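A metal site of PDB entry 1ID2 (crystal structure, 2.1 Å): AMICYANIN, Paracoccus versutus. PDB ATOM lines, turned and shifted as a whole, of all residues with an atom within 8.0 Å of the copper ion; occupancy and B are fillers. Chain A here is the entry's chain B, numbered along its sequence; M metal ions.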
ATOM      1  N   ILE A  26      23.247  -5.051 -28.872  1.00  0.00           N
ATOM      2  CA  ILE A  26      23.000  -6.470 -28.784  1.00  0.00           C
ATOM      3  C   ILE A  26      21.802  -6.613 -27.858  1.00  0.00           C
ATOM      4  O   ILE A  26      21.816  -6.122 -26.736  1.00  0.00           O
ATOM      5  CB  ILE A  26      24.225  -7.262 -28.201  1.00  0.00           C
ATOM      6  CG1 ILE A  26      25.456  -7.087 -29.088  1.00  0.00           C
ATOM      7  CG2 ILE A  26      23.904  -8.727 -28.137  1.00  0.00           C
ATOM      8  CD1 ILE A  26      26.748  -7.519 -28.411  1.00  0.00           C
ATOM      9  N   MET A  29      19.278 -11.769 -28.213  1.00  0.00           N
ATOM     10  CA  MET A  29      20.081 -12.799 -28.852  1.00  0.00           C
ATOM     11  C   MET A  29      20.397 -12.439 -30.299  1.00  0.00           C
ATOM     12  O   MET A  29      20.397 -13.330 -31.163  1.00  0.00           O
ATOM     13  CB  MET A  29      19.362 -14.169 -28.820  1.00  0.00           C
ATOM     14  CG  MET A  29      18.795 -14.616 -27.487  1.00  0.00           C
ATOM     15  SD  MET A  29      20.091 -14.810 -26.294  1.00  0.00           S
ATOM     16  CE  MET A  29      20.821 -16.314 -26.891  1.00  0.00           C
ATOM     17  N   LYS A  30      20.622 -11.172 -30.606  1.00  0.00           N
ATOM     18  CA  LYS A  30      21.072 -10.803 -31.953  1.00  0.00           C
ATOM     19  C   LYS A  30      21.802  -9.492 -31.948  1.00  0.00           C
ATOM     20  O   LYS A  30      21.658  -8.706 -31.012  1.00  0.00           O
ATOM     21  CB  LYS A  30      19.900 -10.705 -32.961  1.00  0.00           C
ATOM     22  CG  LYS A  30      19.032  -9.475 -32.810  1.00  0.00           C
ATOM     23  CD  LYS A  30      17.644  -9.635 -33.431  1.00  0.00           C
ATOM     24  CE  LYS A  30      16.592  -8.917 -32.591  1.00  0.00           C
ATOM     25  NZ  LYS A  30      15.408  -8.400 -33.334  1.00  0.00           N
ATOM     26  N   TYR A  31      22.629  -9.301 -32.966  1.00  0.00           N
ATOM     27  CA  TYR A  31      23.286  -8.023 -33.228  1.00  0.00           C
ATOM     28  C   TYR A  31      22.310  -7.184 -34.012  1.00  0.00           C
ATOM     29  O   TYR A  31      21.944  -7.535 -35.118  1.00  0.00           O
ATOM     30  CB  TYR A  31      24.541  -8.223 -34.076  1.00  0.00           C
ATOM     31  CG  TYR A  31      25.569  -9.077 -33.387  1.00  0.00           C
ATOM     32  CD1 TYR A  31      26.319  -8.583 -32.334  1.00  0.00           C
ATOM     33  CD2 TYR A  31      25.798 -10.384 -33.796  1.00  0.00           C
ATOM     34  CE1 TYR A  31      27.267  -9.349 -31.703  1.00  0.00           C
ATOM     35  CE2 TYR A  31      26.751 -11.179 -33.168  1.00  0.00           C
ATOM     36  CZ  TYR A  31      27.490 -10.634 -32.132  1.00  0.00           C
ATOM     37  OH  TYR A  31      28.522 -11.335 -31.566  1.00  0.00           O
ATOM     38  N   ASN A  48      26.120  -4.348 -25.076  1.00  0.00           N
ATOM     39  CA  ASN A  48      25.185  -5.388 -24.686  1.00  0.00           C
ATOM     40  C   ASN A  48      24.055  -4.793 -23.831  1.00  0.00           C
ATOM     41  O   ASN A  48      24.296  -4.185 -22.768  1.00  0.00           O
ATOM     42  CB  ASN A  48      25.893  -6.489 -23.899  1.00  0.00           C
ATOM     43  CG  ASN A  48      25.000  -7.714 -23.679  1.00  0.00           C
ATOM     44  OD1 ASN A  48      23.922  -7.775 -24.268  1.00  0.00           O
ATOM     45  ND2 ASN A  48      25.416  -8.645 -22.848  1.00  0.00           N
ATOM     46  N   GLU A  50      21.478  -6.623 -22.627  1.00  0.00           N
ATOM     47  CA  GLU A  50      20.759  -7.610 -21.830  1.00  0.00           C
ATOM     48  C   GLU A  50      21.693  -8.397 -20.930  1.00  0.00           C
ATOM     49  O   GLU A  50      22.914  -8.272 -21.032  1.00  0.00           O
ATOM     50  CB  GLU A  50      19.969  -8.559 -22.727  1.00  0.00           C
ATOM     51  CG  GLU A  50      20.786  -9.267 -23.824  1.00  0.00           C
ATOM     52  CD  GLU A  50      19.940 -10.130 -24.775  1.00  0.00           C
ATOM     53  OE1 GLU A  50      18.690 -10.069 -24.718  1.00  0.00           O
ATOM     54  OE2 GLU A  50      20.537 -10.833 -25.610  1.00  0.00           O
ATOM     55  N   MET A  52      22.002 -11.678 -20.691  1.00  0.00           N
ATOM     56  CA  MET A  52      22.659 -12.774 -21.397  1.00  0.00           C
ATOM     57  C   MET A  52      24.027 -12.278 -21.845  1.00  0.00           C
ATOM     58  O   MET A  52      24.112 -11.265 -22.532  1.00  0.00           O
ATOM     59  CB  MET A  52      21.826 -13.175 -22.608  1.00  0.00           C
ATOM     60  CG  MET A  52      22.446 -14.273 -23.456  1.00  0.00           C
ATOM     61  SD  MET A  52      22.445 -15.874 -22.648  1.00  0.00           S
ATOM     62  CE  MET A  52      20.709 -16.220 -22.654  1.00  0.00           C
ATOM     63  N   PRO A  53      25.128 -12.958 -21.431  1.00  0.00           N
ATOM     64  CA  PRO A  53      26.451 -12.555 -21.921  1.00  0.00           C
ATOM     65  C   PRO A  53      26.661 -12.884 -23.398  1.00  0.00           C
ATOM     66  O   PRO A  53      26.201 -13.912 -23.887  1.00  0.00           O
ATOM     67  CB  PRO A  53      27.422 -13.323 -21.027  1.00  0.00           C
ATOM     68  CG  PRO A  53      26.639 -14.465 -20.513  1.00  0.00           C
ATOM     69  CD  PRO A  53      25.248 -13.955 -20.358  1.00  0.00           C
ATOM     70  N   HIS A  54      27.270 -11.944 -24.103  1.00  0.00           N
ATOM     71  CA  HIS A  54      27.509 -12.020 -25.527  1.00  0.00           C
ATOM     72  C   HIS A  54      28.938 -11.505 -25.718  1.00  0.00           C
ATOM     73  O   HIS A  54      29.428 -10.736 -24.913  1.00  0.00           O
ATOM     74  CB  HIS A  54      26.551 -11.069 -26.286  1.00  0.00           C
ATOM     75  CG  HIS A  54      25.110 -11.447 -26.201  1.00  0.00           C
ATOM     76  ND1 HIS A  54      24.603 -12.539 -26.850  1.00  0.00           N
ATOM     77  CD2 HIS A  54      24.108 -10.865 -25.480  1.00  0.00           C
ATOM     78  CE1 HIS A  54      23.336 -12.615 -26.496  1.00  0.00           C
ATOM     79  NE2 HIS A  54      22.993 -11.625 -25.664  1.00  0.00           N
ATOM     80  N   ASN A  55      29.587 -11.894 -26.806  1.00  0.00           N
ATOM     81  CA  ASN A  55      30.873 -11.304 -27.152  1.00  0.00           C
ATOM     82  C   ASN A  55      30.944 -11.136 -28.649  1.00  0.00           C
ATOM     83  O   ASN A  55      29.908 -11.138 -29.310  1.00  0.00           O
ATOM     84  CB  ASN A  55      32.045 -12.153 -26.614  1.00  0.00           C
ATOM     85  CG  ASN A  55      32.299 -13.416 -27.439  1.00  0.00           C
ATOM     86  OD1 ASN A  55      31.385 -13.966 -28.041  1.00  0.00           O
ATOM     87  ND2 ASN A  55      33.508 -13.940 -27.363  1.00  0.00           N
ATOM     88  N   VAL A  56      32.124 -10.771 -29.128  1.00  0.00           N
ATOM     89  CA  VAL A  56      32.402 -10.809 -30.556  1.00  0.00           C
ATOM     90  C   VAL A  56      33.700 -11.594 -30.842  1.00  0.00           C
ATOM     91  O   VAL A  56      34.679 -11.533 -30.065  1.00  0.00           O
ATOM     92  CB  VAL A  56      32.361  -9.346 -31.166  1.00  0.00           C
ATOM     93  CG1 VAL A  56      32.835  -8.338 -30.172  1.00  0.00           C
ATOM     94  CG2 VAL A  56      33.156  -9.254 -32.433  1.00  0.00           C
ATOM     95  N   MET A  72      33.530 -11.669 -22.776  1.00  0.00           N
ATOM     96  CA  MET A  72      32.077 -11.578 -22.600  1.00  0.00           C
ATOM     97  C   MET A  72      31.630 -10.227 -22.038  1.00  0.00           C
ATOM     98  O   MET A  72      32.041  -9.852 -20.937  1.00  0.00           O
ATOM     99  CB  MET A  72      31.547 -12.681 -21.660  1.00  0.00           C
ATOM    100  CG  MET A  72      31.734 -14.128 -22.116  1.00  0.00           C
ATOM    101  SD  MET A  72      31.356 -14.460 -23.834  1.00  0.00           S
ATOM    102  CE  MET A  72      29.596 -14.590 -23.777  1.00  0.00           C
ATOM    103  N   MET A  73      30.728  -9.537 -22.751  1.00  0.00           N
ATOM    104  CA  MET A  73      29.948  -8.444 -22.159  1.00  0.00           C
ATOM    105  C   MET A  73      28.715  -8.949 -21.417  1.00  0.00           C
ATOM    106  O   MET A  73      27.934  -9.760 -21.955  1.00  0.00           O
ATOM    107  CB  MET A  73      29.457  -7.445 -23.223  1.00  0.00           C
ATOM    108  CG  MET A  73      30.547  -6.743 -23.989  1.00  0.00           C
ATOM    109  SD  MET A  73      29.857  -6.072 -25.510  1.00  0.00           S
ATOM    110  CE  MET A  73      30.395  -7.343 -26.668  1.00  0.00           C
ATOM    111  N   PHE A  92      30.999 -13.499 -35.034  1.00  0.00           N
ATOM    112  CA  PHE A  92      29.860 -14.186 -34.447  1.00  0.00           C
ATOM    113  C   PHE A  92      30.032 -14.121 -32.933  1.00  0.00           C
ATOM    114  O   PHE A  92      31.076 -13.679 -32.464  1.00  0.00           O
ATOM    115  CB  PHE A  92      29.822 -15.640 -34.909  1.00  0.00           C
ATOM    116  CG  PHE A  92      31.056 -16.413 -34.567  1.00  0.00           C
ATOM    117  CD1 PHE A  92      32.234 -16.214 -35.272  1.00  0.00           C
ATOM    118  CD2 PHE A  92      31.047 -17.325 -33.523  1.00  0.00           C
ATOM    119  CE1 PHE A  92      33.369 -16.903 -34.941  1.00  0.00           C
ATOM    120  CE2 PHE A  92      32.193 -18.017 -33.184  1.00  0.00           C
ATOM    121  CZ  PHE A  92      33.360 -17.815 -33.897  1.00  0.00           C
ATOM    122  N   CYS A  93      29.034 -14.612 -32.198  1.00  0.00           N
ATOM    123  CA  CYS A  93      29.099 -14.673 -30.739  1.00  0.00           C
ATOM    124  C   CYS A  93      29.502 -16.067 -30.376  1.00  0.00           C
ATOM    125  O   CYS A  93      28.876 -17.041 -30.811  1.00  0.00           O
ATOM    126  CB  CYS A  93      27.749 -14.351 -30.120  1.00  0.00           C
ATOM    127  SG  CYS A  93      27.728 -14.501 -28.318  1.00  0.00           S
ATOM    128  N   THR A  94      30.507 -16.172 -29.531  1.00  0.00           N
ATOM    129  CA  THR A  94      31.125 -17.454 -29.258  1.00  0.00           C
ATOM    130  C   THR A  94      30.151 -18.515 -28.696  1.00  0.00           C
ATOM    131  O   THR A  94      30.032 -19.590 -29.264  1.00  0.00           O
ATOM    132  CB  THR A  94      32.361 -17.269 -28.375  1.00  0.00           C
ATOM    133  OG1 THR A  94      33.367 -16.565 -29.124  1.00  0.00           O
ATOM    134  CG2 THR A  94      32.922 -18.608 -27.916  1.00  0.00           C
ATOM    135  N   PRO A  95      29.367 -18.180 -27.651  1.00  0.00           N
ATOM    136  CA  PRO A  95      28.402 -19.186 -27.153  1.00  0.00           C
ATOM    137  C   PRO A  95      27.128 -19.336 -28.000  1.00  0.00           C
ATOM    138  O   PRO A  95      26.409 -20.342 -27.891  1.00  0.00           O
ATOM    139  CB  PRO A  95      28.094 -18.705 -25.750  1.00  0.00           C
ATOM    140  CG  PRO A  95      28.325 -17.223 -25.811  1.00  0.00           C
ATOM    141  CD  PRO A  95      29.504 -17.052 -26.714  1.00  0.00           C
ATOM    142  N   HIS A  96      26.869 -18.330 -28.834  1.00  0.00           N
ATOM    143  CA  HIS A  96      25.692 -18.283 -29.698  1.00  0.00           C
ATOM    144  C   HIS A  96      26.088 -18.009 -31.145  1.00  0.00           C
ATOM    145  O   HIS A  96      25.817 -16.914 -31.666  1.00  0.00           O
ATOM    146  CB  HIS A  96      24.722 -17.189 -29.235  1.00  0.00           C
ATOM    147  CG  HIS A  96      24.514 -17.156 -27.747  1.00  0.00           C
ATOM    148  ND1 HIS A  96      24.822 -16.030 -27.007  1.00  0.00           N
ATOM    149  CD2 HIS A  96      24.171 -18.155 -26.909  1.00  0.00           C
ATOM    150  CE1 HIS A  96      24.673 -16.387 -25.751  1.00  0.00           C
ATOM    151  NE2 HIS A  96      24.290 -17.663 -25.641  1.00  0.00           N
ATOM    152  N   PRO A  97      26.617 -19.012 -31.857  1.00  0.00           N
ATOM    153  CA  PRO A  97      27.219 -18.748 -33.174  1.00  0.00           C
ATOM    154  C   PRO A  97      26.172 -18.454 -34.223  1.00  0.00           C
ATOM    155  O   PRO A  97      26.505 -18.047 -35.337  1.00  0.00           O
ATOM    156  CB  PRO A  97      27.982 -20.032 -33.499  1.00  0.00           C
ATOM    157  CG  PRO A  97      28.099 -20.771 -32.189  1.00  0.00           C
ATOM    158  CD  PRO A  97      26.866 -20.403 -31.423  1.00  0.00           C
ATOM    159  N   PHE A  98      24.901 -18.636 -33.862  1.00  0.00           N
ATOM    160  CA  PHE A  98      23.800 -18.253 -34.719  1.00  0.00           C
ATOM    161  C   PHE A  98      23.620 -16.727 -34.742  1.00  0.00           C
ATOM    162  O   PHE A  98      22.978 -16.185 -35.660  1.00  0.00           O
ATOM    163  CB  PHE A  98      22.496 -18.979 -34.285  1.00  0.00           C
ATOM    164  CG  PHE A  98      22.125 -18.765 -32.848  1.00  0.00           C
ATOM    165  CD1 PHE A  98      21.436 -17.606 -32.456  1.00  0.00           C
ATOM    166  CD2 PHE A  98      22.480 -19.689 -31.865  1.00  0.00           C
ATOM    167  CE1 PHE A  98      21.132 -17.368 -31.121  1.00  0.00           C
ATOM    168  CE2 PHE A  98      22.161 -19.452 -30.511  1.00  0.00           C
ATOM    169  CZ  PHE A  98      21.500 -18.292 -30.144  1.00  0.00           C
ATOM    170  N   MET A  99      24.275 -16.046 -33.801  1.00  0.00           N
ATOM    171  CA  MET A  99      24.452 -14.587 -33.823  1.00  0.00           C
ATOM    172  C   MET A  99      25.642 -14.187 -34.693  1.00  0.00           C
ATOM    173  O   MET A  99      26.790 -14.461 -34.355  1.00  0.00           O
ATOM    174  CB  MET A  99      24.690 -14.057 -32.403  1.00  0.00           C
ATOM    175  CG  MET A  99      23.491 -14.152 -31.485  1.00  0.00           C
ATOM    176  SD  MET A  99      23.901 -13.665 -29.807  1.00  0.00           S
ATOM    177  CE  MET A  99      24.106 -11.864 -30.088  1.00  0.00           C
HETATM  178 CU    CU M   1      25.656 -14.199 -27.760  1.00  0.00          CU
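Residues that only touch the copper ion: Pro 53 (3.9 Å). Of the 21 residues printed, 5 come within 4 Å of the copper ion.
The backbone carbonyl oxygen of Met 52 lies close to a ring nitrogen (NE2) of His 54 (3.3 Å). NE2 of His 54 lies within hydrogen-bond range of OE2 of Glu 50. The backbone carbonyl oxygen (O) of His 54 lies within hydrogen-bond range of the backbone NH (N) of Met 73 (2.8 Å). SG of Cys 93 lies close to N of Asn 55 (3.5 Å). The side-chain hydroxyl (OH) of Tyr 31 is in hydrogen-bond range of the backbone NH (N) of Cys 93, 3.4 Å away.
The copper ion is bound by a ring nitrogen (ND1) of His 96, a ring nitrogen (ND1) of His 54, the side-chain sulfur (SG) of Cys 93 and the side-chain sulfur (SD) of Met 99.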
